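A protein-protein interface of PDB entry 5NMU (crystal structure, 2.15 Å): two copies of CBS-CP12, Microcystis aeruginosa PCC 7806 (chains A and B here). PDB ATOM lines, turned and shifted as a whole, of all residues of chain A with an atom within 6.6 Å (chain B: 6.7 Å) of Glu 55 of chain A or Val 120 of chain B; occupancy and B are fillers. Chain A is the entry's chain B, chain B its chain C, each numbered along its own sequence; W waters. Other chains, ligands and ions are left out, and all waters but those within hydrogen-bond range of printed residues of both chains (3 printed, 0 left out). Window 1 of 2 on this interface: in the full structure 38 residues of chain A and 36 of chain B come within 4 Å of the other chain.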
ATOM      1  N   MET A  31     -10.096  21.592 -13.231  1.00  0.00           N
ATOM      2  CA  MET A  31     -10.893  20.416 -12.977  1.00  0.00           C
ATOM      3  C   MET A  31     -11.703  20.559 -11.698  1.00  0.00           C
ATOM      4  O   MET A  31     -12.857  20.150 -11.709  1.00  0.00           O
ATOM      5  CB  MET A  31     -10.020  19.144 -12.939  1.00  0.00           C
ATOM      6  CG  MET A  31      -9.478  18.760 -14.304  1.00  0.00           C
ATOM      7  SD  MET A  31      -8.079  17.635 -14.290  1.00  0.00           S
ATOM      8  CE  MET A  31      -8.959  16.132 -14.695  1.00  0.00           C
ATOM      9  N   LEU A  36     -14.530  18.499 -13.466  1.00  0.00           N
ATOM     10  CA  LEU A  36     -14.201  17.741 -14.651  1.00  0.00           C
ATOM     11  C   LEU A  36     -13.214  16.651 -14.284  1.00  0.00           C
ATOM     12  O   LEU A  36     -12.163  16.943 -13.687  1.00  0.00           O
ATOM     13  CB  LEU A  36     -13.544  18.637 -15.713  1.00  0.00           C
ATOM     14  CG  LEU A  36     -14.349  19.867 -16.123  1.00  0.00           C
ATOM     15  CD1 LEU A  36     -13.608  20.671 -17.187  1.00  0.00           C
ATOM     16  CD2 LEU A  36     -15.762  19.512 -16.600  1.00  0.00           C
ATOM     17  N   ARG A  37     -13.549  15.417 -14.663  1.00  0.00           N
ATOM     18  CA  ARG A  37     -12.631  14.263 -14.529  1.00  0.00           C
ATOM     19  C   ARG A  37     -11.726  13.973 -15.735  1.00  0.00           C
ATOM     20  O   ARG A  37     -10.837  13.125 -15.658  1.00  0.00           O
ATOM     21  CB  ARG A  37     -13.445  13.042 -14.184  1.00  0.00           C
ATOM     22  CG  ARG A  37     -14.301  13.254 -12.933  1.00  0.00           C
ATOM     23  CD  ARG A  37     -15.251  12.082 -12.697  1.00  0.00           C
ATOM     24  NE  ARG A  37     -15.924  12.216 -11.408  1.00  0.00           N
ATOM     25  CZ  ARG A  37     -16.911  13.070 -11.175  1.00  0.00           C
ATOM     26  NH1 ARG A  37     -17.378  13.851 -12.144  1.00  0.00           N
ATOM     27  NH2 ARG A  37     -17.429  13.157  -9.958  1.00  0.00           N
ATOM     28  N   GLY A  38     -11.937  14.676 -16.841  1.00  0.00           N
ATOM     29  CA  GLY A  38     -10.922  14.795 -17.909  1.00  0.00           C
ATOM     30  C   GLY A  38     -10.849  16.219 -18.488  1.00  0.00           C
ATOM     31  O   GLY A  38     -11.821  16.977 -18.458  1.00  0.00           O
ATOM     32  N   LEU A  39      -9.669  16.596 -18.974  1.00  0.00           N
ATOM     33  CA  LEU A  39      -9.483  17.739 -19.855  1.00  0.00           C
ATOM     34  C   LEU A  39      -8.915  17.276 -21.179  1.00  0.00           C
ATOM     35  O   LEU A  39      -8.022  16.444 -21.235  1.00  0.00           O
ATOM     36  CB  LEU A  39      -8.481  18.700 -19.267  1.00  0.00           C
ATOM     37  CG  LEU A  39      -8.859  19.392 -17.967  1.00  0.00           C
ATOM     38  CD1 LEU A  39      -7.611  20.067 -17.400  1.00  0.00           C
ATOM     39  CD2 LEU A  39     -10.006  20.365 -18.259  1.00  0.00           C
ATOM     40  N   VAL A  53      -6.119  14.287 -20.617  1.00  0.00           N
ATOM     41  CA  VAL A  53      -5.517  14.123 -19.310  1.00  0.00           C
ATOM     42  C   VAL A  53      -6.658  13.888 -18.350  1.00  0.00           C
ATOM     43  O   VAL A  53      -7.633  14.600 -18.396  1.00  0.00           O
ATOM     44  CB  VAL A  53      -4.584  15.303 -18.922  1.00  0.00           C
ATOM     45  CG1 VAL A  53      -5.293  16.652 -18.792  1.00  0.00           C
ATOM     46  CG2 VAL A  53      -3.806  14.923 -17.658  1.00  0.00           C
ATOM     47  N   THR A  54      -6.556  12.861 -17.513  1.00  0.00           N
ATOM     48  CA  THR A  54      -7.689  12.421 -16.707  1.00  0.00           C
ATOM     49  C   THR A  54      -7.344  12.431 -15.251  1.00  0.00           C
ATOM     50  O   THR A  54      -6.189  12.562 -14.869  1.00  0.00           O
ATOM     51  CB  THR A  54      -8.104  10.947 -17.028  1.00  0.00           C
ATOM     52  OG1 THR A  54      -7.168  10.090 -16.415  1.00  0.00           O
ATOM     53  CG2 THR A  54      -8.135  10.633 -18.562  1.00  0.00           C
ATOM     54  N   GLU A  55      -8.370  12.217 -14.438  1.00  0.00           N
ATOM     55  CA  GLU A  55      -8.216  12.153 -12.989  1.00  0.00           C
ATOM     56  C   GLU A  55      -7.299  11.014 -12.562  1.00  0.00           C
ATOM     57  O   GLU A  55      -6.477  11.175 -11.615  1.00  0.00           O
ATOM     58  CB  GLU A  55      -9.569  12.062 -12.300  1.00  0.00           C
ATOM     59  CG  GLU A  55     -10.314  10.760 -12.555  1.00  0.00           C
ATOM     60  CD  GLU A  55     -11.688  10.740 -11.963  1.00  0.00           C
ATOM     61  OE1 GLU A  55     -12.058  11.680 -11.195  1.00  0.00           O
ATOM     62  OE2 GLU A  55     -12.390   9.761 -12.285  1.00  0.00           O
ATOM     63  N   THR A  56      -7.401   9.881 -13.275  1.00  0.00           N
ATOM     64  CA  THR A  56      -6.527   8.741 -12.998  1.00  0.00           C
ATOM     65  C   THR A  56      -5.062   9.048 -13.340  1.00  0.00           C
ATOM     66  O   THR A  56      -4.155   8.735 -12.537  1.00  0.00           O
ATOM     67  CB  THR A  56      -7.075   7.430 -13.636  1.00  0.00           C
ATOM     68  OG1 THR A  56      -8.472   7.298 -13.318  1.00  0.00           O
ATOM     69  CG2 THR A  56      -6.425   6.242 -13.013  1.00  0.00           C
ATOM     70  N   ASP A  57      -4.820   9.734 -14.461  1.00  0.00           N
ATOM     71  CA  ASP A  57      -3.463  10.176 -14.758  1.00  0.00           C
ATOM     72  C   ASP A  57      -2.918  10.997 -13.613  1.00  0.00           C
ATOM     73  O   ASP A  57      -1.795  10.793 -13.171  1.00  0.00           O
ATOM     74  CB  ASP A  57      -3.381  11.048 -16.005  1.00  0.00           C
ATOM     75  CG  ASP A  57      -3.801  10.326 -17.273  1.00  0.00           C
ATOM     76  OD1 ASP A  57      -3.429   9.161 -17.395  1.00  0.00           O
ATOM     77  OD2 ASP A  57      -4.475  10.959 -18.139  1.00  0.00           O
ATOM     78  N   ILE A  58      -3.718  11.949 -13.133  1.00  0.00           N
ATOM     79  CA  ILE A  58      -3.238  12.850 -12.088  1.00  0.00           C
ATOM     80  C   ILE A  58      -2.989  12.102 -10.798  1.00  0.00           C
ATOM     81  O   ILE A  58      -1.945  12.264 -10.207  1.00  0.00           O
ATOM     82  CB  ILE A  58      -4.170  14.063 -11.924  1.00  0.00           C
ATOM     83  CG1 ILE A  58      -4.085  14.896 -13.202  1.00  0.00           C
ATOM     84  CG2 ILE A  58      -3.740  14.933 -10.717  1.00  0.00           C
ATOM     85  CD1 ILE A  58      -5.155  15.969 -13.324  1.00  0.00           C
ATOM     86  N   VAL A  59      -3.917  11.253 -10.377  1.00  0.00           N
ATOM     87  CA  VAL A  59      -3.788  10.548  -9.090  1.00  0.00           C
ATOM     88  C   VAL A  59      -2.652   9.541  -9.154  1.00  0.00           C
ATOM     89  O   VAL A  59      -1.821   9.514  -8.256  1.00  0.00           O
ATOM     90  CB  VAL A  59      -5.112   9.875  -8.674  1.00  0.00           C
ATOM     91  CG1 VAL A  59      -4.964   8.927  -7.466  1.00  0.00           C
ATOM     92  CG2 VAL A  59      -6.172  10.925  -8.403  1.00  0.00           C
ATOM     93  N   TYR A  60      -2.610   8.720 -10.217  1.00  0.00           N
ATOM     94  CA  TYR A  60      -1.601   7.658 -10.320  1.00  0.00           C
ATOM     95  C   TYR A  60      -0.227   8.200 -10.635  1.00  0.00           C
ATOM     96  O   TYR A  60       0.739   7.708 -10.123  1.00  0.00           O
ATOM     97  CB  TYR A  60      -1.939   6.675 -11.434  1.00  0.00           C
ATOM     98  CG  TYR A  60      -3.075   5.719 -11.217  1.00  0.00           C
ATOM     99  CD1 TYR A  60      -3.947   5.803 -10.116  1.00  0.00           C
ATOM    100  CD2 TYR A  60      -3.289   4.696 -12.154  1.00  0.00           C
ATOM    101  CE1 TYR A  60      -4.985   4.890  -9.936  1.00  0.00           C
ATOM    102  CE2 TYR A  60      -4.344   3.809 -12.010  1.00  0.00           C
ATOM    103  CZ  TYR A  60      -5.205   3.905 -10.914  1.00  0.00           C
ATOM    104  OH  TYR A  60      -6.215   2.959 -10.784  1.00  0.00           O
ATOM    105  N   ARG A 104     -11.578   5.181 -19.818  1.00  0.00           N
ATOM    106  CA  ARG A 104     -12.820   5.519 -19.178  1.00  0.00           C
ATOM    107  C   ARG A 104     -13.476   6.727 -19.732  1.00  0.00           C
ATOM    108  O   ARG A 104     -14.598   7.018 -19.352  1.00  0.00           O
ATOM    109  CB  ARG A 104     -12.617   5.616 -17.661  1.00  0.00           C
ATOM    110  CG  ARG A 104     -12.567   4.223 -17.034  1.00  0.00           C
ATOM    111  CD  ARG A 104     -11.715   4.134 -15.771  1.00  0.00           C
ATOM    112  NE  ARG A 104     -10.482   4.889 -15.890  1.00  0.00           N
ATOM    113  CZ  ARG A 104      -9.283   4.425 -16.216  1.00  0.00           C
ATOM    114  NH1 ARG A 104      -9.060   3.149 -16.415  1.00  0.00           N
ATOM    115  NH2 ARG A 104      -8.265   5.277 -16.308  1.00  0.00           N
ATOM    116  N   ARG A 105     -12.801   7.407 -20.648  1.00  0.00           N
ATOM    117  CA  ARG A 105     -13.273   8.654 -21.165  1.00  0.00           C
ATOM    118  C   ARG A 105     -12.494   9.080 -22.422  1.00  0.00           C
ATOM    119  O   ARG A 105     -11.364   8.648 -22.661  1.00  0.00           O
ATOM    120  CB  ARG A 105     -13.290   9.736 -20.093  1.00  0.00           C
ATOM    121  CG  ARG A 105     -11.987  10.057 -19.455  1.00  0.00           C
ATOM    122  CD  ARG A 105     -12.241  10.934 -18.228  1.00  0.00           C
ATOM    123  NE  ARG A 105     -12.611  10.110 -17.102  1.00  0.00           N
ATOM    124  CZ  ARG A 105     -13.783  10.060 -16.495  1.00  0.00           C
ATOM    125  NH1 ARG A 105     -14.818  10.822 -16.831  1.00  0.00           N
ATOM    126  NH2 ARG A 105     -13.898   9.218 -15.489  1.00  0.00           N
ATOM    127  N   ARG B  37     -21.036   6.235  -8.744  1.00  0.00           N
ATOM    128  CA  ARG B  37     -20.157   5.500  -9.639  1.00  0.00           C
ATOM    129  C   ARG B  37     -19.641   4.206  -9.027  1.00  0.00           C
ATOM    130  O   ARG B  37     -19.021   3.422  -9.709  1.00  0.00           O
ATOM    131  CB  ARG B  37     -18.994   6.386 -10.053  1.00  0.00           C
ATOM    132  CG  ARG B  37     -19.453   7.634 -10.771  1.00  0.00           C
ATOM    133  CD  ARG B  37     -18.304   8.620 -10.985  1.00  0.00           C
ATOM    134  NE  ARG B  37     -18.753   9.718 -11.816  1.00  0.00           N
ATOM    135  CZ  ARG B  37     -19.555  10.709 -11.398  1.00  0.00           C
ATOM    136  NH1 ARG B  37     -19.991  10.778 -10.125  1.00  0.00           N
ATOM    137  NH2 ARG B  37     -19.923  11.657 -12.266  1.00  0.00           N
ATOM    138  N   GLU B  55     -19.103   1.614 -11.944  1.00  0.00           N
ATOM    139  CA  GLU B  55     -19.493   2.015 -13.281  1.00  0.00           C
ATOM    140  C   GLU B  55     -18.677   1.263 -14.328  1.00  0.00           C
ATOM    141  O   GLU B  55     -19.217   0.849 -15.329  1.00  0.00           O
ATOM    142  CB  GLU B  55     -19.342   3.523 -13.449  1.00  0.00           C
ATOM    143  CG  GLU B  55     -17.936   4.050 -13.296  1.00  0.00           C
ATOM    144  CD  GLU B  55     -17.828   5.560 -13.545  1.00  0.00           C
ATOM    145  OE1 GLU B  55     -18.867   6.195 -13.772  1.00  0.00           O
ATOM    146  OE2 GLU B  55     -16.684   6.097 -13.485  1.00  0.00           O
ATOM    147  N   ALA B  95      -3.831   7.279  -2.797  1.00  0.00           N
ATOM    148  CA  ALA B  95      -3.497   7.467  -4.208  1.00  0.00           C
ATOM    149  C   ALA B  95      -2.634   6.339  -4.677  1.00  0.00           C
ATOM    150  O   ALA B  95      -2.849   5.792  -5.770  1.00  0.00           O
ATOM    151  CB  ALA B  95      -2.743   8.784  -4.431  1.00  0.00           C
ATOM    152  N   PHE B  98      -4.385   2.807  -4.755  1.00  0.00           N
ATOM    153  CA  PHE B  98      -5.171   2.814  -5.983  1.00  0.00           C
ATOM    154  C   PHE B  98      -4.353   2.573  -7.244  1.00  0.00           C
ATOM    155  O   PHE B  98      -4.748   1.791  -8.079  1.00  0.00           O
ATOM    156  CB  PHE B  98      -5.954   4.111  -6.098  1.00  0.00           C
ATOM    157  CG  PHE B  98      -7.161   4.206  -5.198  1.00  0.00           C
ATOM    158  CD1 PHE B  98      -7.400   3.295  -4.146  1.00  0.00           C
ATOM    159  CD2 PHE B  98      -8.043   5.228  -5.386  1.00  0.00           C
ATOM    160  CE1 PHE B  98      -8.518   3.401  -3.364  1.00  0.00           C
ATOM    161  CE2 PHE B  98      -9.146   5.366  -4.593  1.00  0.00           C
ATOM    162  CZ  PHE B  98      -9.395   4.451  -3.568  1.00  0.00           C
ATOM    163  N   ILE B 103      -7.261   0.251  -9.068  1.00  0.00           N
ATOM    164  CA  ILE B 103      -8.643   0.559  -8.821  1.00  0.00           C
ATOM    165  C   ILE B 103      -8.763   2.086  -8.736  1.00  0.00           C
ATOM    166  O   ILE B 103      -7.758   2.774  -8.620  1.00  0.00           O
ATOM    167  CB  ILE B 103      -9.150  -0.104  -7.541  1.00  0.00           C
ATOM    168  CG1 ILE B 103      -8.358   0.415  -6.307  1.00  0.00           C
ATOM    169  CG2 ILE B 103      -9.133  -1.641  -7.726  1.00  0.00           C
ATOM    170  CD1 ILE B 103      -9.017   0.086  -4.992  1.00  0.00           C
ATOM    171  N   ARG B 104     -10.000   2.549  -8.767  1.00  0.00           N
ATOM    172  CA  ARG B 104     -10.370   3.939  -8.750  1.00  0.00           C
ATOM    173  C   ARG B 104     -11.256   4.342  -7.557  1.00  0.00           C
ATOM    174  O   ARG B 104     -11.472   5.543  -7.342  1.00  0.00           O
ATOM    175  CB  ARG B 104     -11.067   4.276 -10.080  1.00  0.00           C
ATOM    176  CG  ARG B 104     -10.057   4.306 -11.217  1.00  0.00           C
ATOM    177  CD  ARG B 104     -10.579   4.033 -12.607  1.00  0.00           C
ATOM    178  NE  ARG B 104     -11.368   2.820 -12.718  1.00  0.00           N
ATOM    179  CZ  ARG B 104     -10.931   1.590 -13.016  1.00  0.00           C
ATOM    180  NH1 ARG B 104      -9.674   1.307 -13.222  1.00  0.00           N
ATOM    181  NH2 ARG B 104     -11.788   0.594 -13.045  1.00  0.00           N
ATOM    182  N   ARG B 105     -11.828   3.364  -6.847  1.00  0.00           N
ATOM    183  CA  ARG B 105     -12.639   3.631  -5.695  1.00  0.00           C
ATOM    184  C   ARG B 105     -12.678   2.439  -4.722  1.00  0.00           C
ATOM    185  O   ARG B 105     -12.346   1.316  -5.090  1.00  0.00           O
ATOM    186  CB  ARG B 105     -14.030   4.065  -6.115  1.00  0.00           C
ATOM    187  CG  ARG B 105     -14.775   3.106  -7.010  1.00  0.00           C
ATOM    188  CD  ARG B 105     -15.922   3.834  -7.668  1.00  0.00           C
ATOM    189  NE  ARG B 105     -15.436   4.452  -8.866  1.00  0.00           N
ATOM    190  CZ  ARG B 105     -15.380   5.743  -9.168  1.00  0.00           C
ATOM    191  NH1 ARG B 105     -15.840   6.687  -8.386  1.00  0.00           N
ATOM    192  NH2 ARG B 105     -14.861   6.076 -10.345  1.00  0.00           N
ATOM    193  N   ILE B 118     -14.266   6.341  -1.030  1.00  0.00           N
ATOM    194  CA  ILE B 118     -13.262   7.250  -1.497  1.00  0.00           C
ATOM    195  C   ILE B 118     -12.875   6.844  -2.920  1.00  0.00           C
ATOM    196  O   ILE B 118     -12.709   5.650  -3.185  1.00  0.00           O
ATOM    197  CB  ILE B 118     -12.061   7.295  -0.536  1.00  0.00           C
ATOM    198  CG1 ILE B 118     -11.074   8.392  -0.985  1.00  0.00           C
ATOM    199  CG2 ILE B 118     -11.365   5.946  -0.383  1.00  0.00           C
ATOM    200  CD1 ILE B 118     -10.125   8.759   0.120  1.00  0.00           C
ATOM    201  N   SER B 119     -12.745   7.839  -3.809  1.00  0.00           N
ATOM    202  CA  SER B 119     -12.454   7.605  -5.243  1.00  0.00           C
ATOM    203  C   SER B 119     -11.301   8.474  -5.719  1.00  0.00           C
ATOM    204  O   SER B 119     -10.925   9.437  -5.033  1.00  0.00           O
ATOM    205  CB  SER B 119     -13.688   7.894  -6.138  1.00  0.00           C
ATOM    206  OG  SER B 119     -13.935   9.320  -6.267  1.00  0.00           O
ATOM    207  N   VAL B 120     -10.780   8.159  -6.913  1.00  0.00           N
ATOM    208  CA  VAL B 120      -9.847   9.075  -7.596  1.00  0.00           C
ATOM    209  C   VAL B 120     -10.434  10.509  -7.729  1.00  0.00           C
ATOM    210  O   VAL B 120      -9.674  11.462  -7.689  1.00  0.00           O
ATOM    211  CB  VAL B 120      -9.316   8.592  -8.987  1.00  0.00           C
ATOM    212  CG1 VAL B 120      -8.483   7.351  -8.858  1.00  0.00           C
ATOM    213  CG2 VAL B 120     -10.446   8.366  -9.961  1.00  0.00           C
ATOM    214  N   SER B 121     -11.751  10.632  -7.890  1.00  0.00           N
ATOM    215  CA  SER B 121     -12.432  11.923  -7.944  1.00  0.00           C
ATOM    216  C   SER B 121     -12.291  12.721  -6.610  1.00  0.00           C
ATOM    217  O   SER B 121     -12.000  13.904  -6.620  1.00  0.00           O
ATOM    218  CB  SER B 121     -13.930  11.781  -8.270  1.00  0.00           C
ATOM    219  OG  SER B 121     -14.196  11.157  -9.511  1.00  0.00           O
ATOM    220  N   ASP B 122     -12.530  12.066  -5.485  1.00  0.00           N
ATOM    221  CA  ASP B 122     -12.309  12.650  -4.178  1.00  0.00           C
ATOM    222  C   ASP B 122     -10.882  13.158  -4.027  1.00  0.00           C
ATOM    223  O   ASP B 122     -10.658  14.273  -3.578  1.00  0.00           O
ATOM    224  CB  ASP B 122     -12.606  11.661  -3.046  1.00  0.00           C
ATOM    225  CG  ASP B 122     -14.062  11.216  -3.006  1.00  0.00           C
ATOM    226  OD1 ASP B 122     -14.988  12.029  -3.191  1.00  0.00           O
ATOM    227  OD2 ASP B 122     -14.287  10.030  -2.782  1.00  0.00           O
ATOM    228  N   ILE B 123      -9.925  12.348  -4.427  1.00  0.00           N
ATOM    229  CA  ILE B 123      -8.524  12.729  -4.342  1.00  0.00           C
ATOM    230  C   ILE B 123      -8.264  13.968  -5.217  1.00  0.00           C
ATOM    231  O   ILE B 123      -7.715  14.943  -4.723  1.00  0.00           O
ATOM    232  CB  ILE B 123      -7.570  11.569  -4.758  1.00  0.00           C
ATOM    233  CG1 ILE B 123      -7.738  10.386  -3.798  1.00  0.00           C
ATOM    234  CG2 ILE B 123      -6.122  12.010  -4.705  1.00  0.00           C
ATOM    235  CD1 ILE B 123      -7.066   9.126  -4.191  1.00  0.00           C
ATOM    236  N   LEU B 124      -8.673  13.924  -6.484  1.00  0.00           N
ATOM    237  CA  LEU B 124      -8.433  15.030  -7.405  1.00  0.00           C
ATOM    238  C   LEU B 124      -9.055  16.314  -6.899  1.00  0.00           C
ATOM    239  O   LEU B 124      -8.385  17.331  -6.895  1.00  0.00           O
ATOM    240  CB  LEU B 124      -8.979  14.753  -8.788  1.00  0.00           C
ATOM    241  CG  LEU B 124      -8.962  15.870  -9.823  1.00  0.00           C
ATOM    242  CD1 LEU B 124      -7.521  16.189 -10.214  1.00  0.00           C
ATOM    243  CD2 LEU B 124      -9.724  15.453 -11.065  1.00  0.00           C
ATOM    244  N   PHE B 125     -10.316  16.263  -6.462  1.00  0.00           N
ATOM    245  CA  PHE B 125     -11.076  17.473  -6.058  1.00  0.00           C
ATOM    246  C   PHE B 125     -10.787  17.984  -4.630  1.00  0.00           C
ATOM    247  O   PHE B 125     -10.958  19.184  -4.374  1.00  0.00           O
ATOM    248  CB  PHE B 125     -12.581  17.262  -6.202  1.00  0.00           C
ATOM    249  CG  PHE B 125     -13.031  16.859  -7.601  1.00  0.00           C
ATOM    250  CD1 PHE B 125     -12.534  17.506  -8.757  1.00  0.00           C
ATOM    251  CD2 PHE B 125     -14.003  15.868  -7.766  1.00  0.00           C
ATOM    252  CE1 PHE B 125     -12.988  17.166 -10.016  1.00  0.00           C
ATOM    253  CE2 PHE B 125     -14.448  15.499  -9.039  1.00  0.00           C
ATOM    254  CZ  PHE B 125     -13.941  16.146 -10.164  1.00  0.00           C
HETATM  255  O   HOH W   1     -14.684   8.717 -11.217  1.00  0.00           O
HETATM  256  O   HOH W   2      -7.466   2.698 -13.321  1.00  0.00           O
HETATM  257  O   HOH W   3     -15.724   8.601 -13.537  1.00  0.00           O
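Water W2 lies within hydrogen-bond range of the guanidinium group (NH1) of Arg 104 of chain B and the side-chain hydroxyl (OH) of Tyr 60 of chain A. Water W3 bridges OE2 of Glu 55 of chain B (2.7 Å) and NH2 of Arg 105 of chain A (2.7 Å). Water W1 lies within hydrogen-bond range of OE2 of Glu 55 of chain A (2.7 Å), NH2 of Arg 105 of chain B (2.8 Å) and OG of Ser 121 of chain B (3.0 Å).
Of the 15 printed residues of chain A, 9 touch a printed residue of chain B. Hydrophobic or aromatic side chains of chain A within 4 Å of the printed part of chain B: Met 31, Ile 58, Val 59 and Tyr 60. Printed residues of chain B that touch a printed residue of chain A: Arg 37, Ala 95, Phe 98, Ile 103, Arg 104, Val 120, Ser 121, Ile 123, Leu 124 and Phe 125.
The backbone carbonyl oxygen of Phe 98 of chain B lies within hydrogen-bond range of the backbone NH of Ile 103 of chain B (3.1 Å). NE of Arg 37 of chain A is in salt-bridge range of OE1 of Glu 55 of chain A, at 3.9 Å. The guanidinium group (NH2) of Arg 105 of chain A is in salt-bridge range of the side-chain carboxylate (OE2) of Glu 55 of chain A (3.6 Å). N of Val 120 of chain B is in hydrogen-bond range of O of Arg 104 of chain B (2.7 Å). The backbone NH (N) of Ser 121 of chain B sits at hydrogen-bond distance from the side-chain hydroxyl (OG) of Ser 119 of chain B (3.0 Å). The backbone NH (N) of Thr 56 of chain A sits at hydrogen-bond distance from the side-chain hydroxyl (OG1) of Thr 54 of chain A, at 3.2 Å.
The side-chain hydroxyl (OG) of Ser 121 of chain B lies within hydrogen-bond range of the side-chain carboxylate (OE1) of Glu 55 of chain A (2.8 Å). O of Phe 98 of chain B is in hydrogen-bond range of OH of Tyr 60 of chain A. NE of Arg 37 of chain A sits at hydrogen-bond distance from OG of Ser 121 of chain B (2.8 Å). The backbone carbonyl oxygen of Ile 103 of chain B sits at hydrogen-bond distance from the side-chain hydroxyl of Tyr 60 of chain A (2.7 Å). The guanidinium group (NH1) of Arg 37 of chain A sits close to the guanidinium group (NH2) of Arg 37 of chain B.
Among the printed residues, merely in contact across the chains: Glu 55 of chain A with Val 120 of chain B (3.3 Å), Arg 104 of chain A with Arg 104 of chain B (3.3 Å), Met 31 of chain A with Phe 125 of chain B (3.4 Å), Glu 55 of chain A with Leu 124 of chain B (3.6 Å), Val 59 of chain A with Val 120 of chain B (3.6 Å), Val 59 of chain A with Ala 95 of chain B (3.8 Å), Leu 36 of chain A with Phe 125 of chain B (3.8 Å), Met 31 of chain A with Leu 124 of chain B (3.8 Å), Val 59 of chain A with Ile 123 of chain B (3.9 Å), Leu 36 of chain A with Leu 124 of chain B (3.9 Å), Arg 37 of chain A with Phe 125 of chain B (3.9 Å), Ile 58 of chain A with Leu 124 of chain B (3.9 Å) and Thr 56 of chain A with Arg 104 of chain B (3.95 Å).
Of the printed residues of chain B, Leu 36 of chain A touches Leu 124 and Phe 125. Of chain B, only Val 120 (3.3 Å), Ser 121 (2.8 Å) and Leu 124 (3.6 Å) come within 4 Å of Glu 55 of chain A. Of the printed residues of chain B, Val 59 of chain A touches Ala 95, Val 120 and Ile 123. Of the printed residues of chain A, Arg 37 of chain B touches Arg 37 (3.4 Å). Glu 55 of chain B touches none of the printed residues of chain A. Of the printed residues of chain A, Phe 98 of chain B touches Tyr 60 (3.3 Å). Of the printed residues of chain A, Ile 103 of chain B touches Tyr 60. Of chain A, only Glu 55 (3.3 Å) and Val 59 (3.6 Å) come within 4 Å of Val 120 of chain B. Asp 122 of chain B touches none of the printed residues of chain A. The nearest residue of chain B that does not touch Glu 55 of chain A is Arg 105 of chain B (4.8 Å). The nearest residue of chain A that does not touch Val 120 of chain B is Thr 56 of chain A (4.04 Å). The nearest printed residue of chain A that does not touch Leu 124 of chain B is Val 59 of chain A (4.4 Å).
Arg 37 of chain B touches its own counterpart, Arg 37 of chain A. Arg 104 of chain B touches its own counterpart, Arg 104 of chain A. Positions printed for both chains: 37, 55, 104 and 105. Of the 18 pairs that touch across the chains among the printed residues, 2 have their exchanged pair printed and touching as well.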
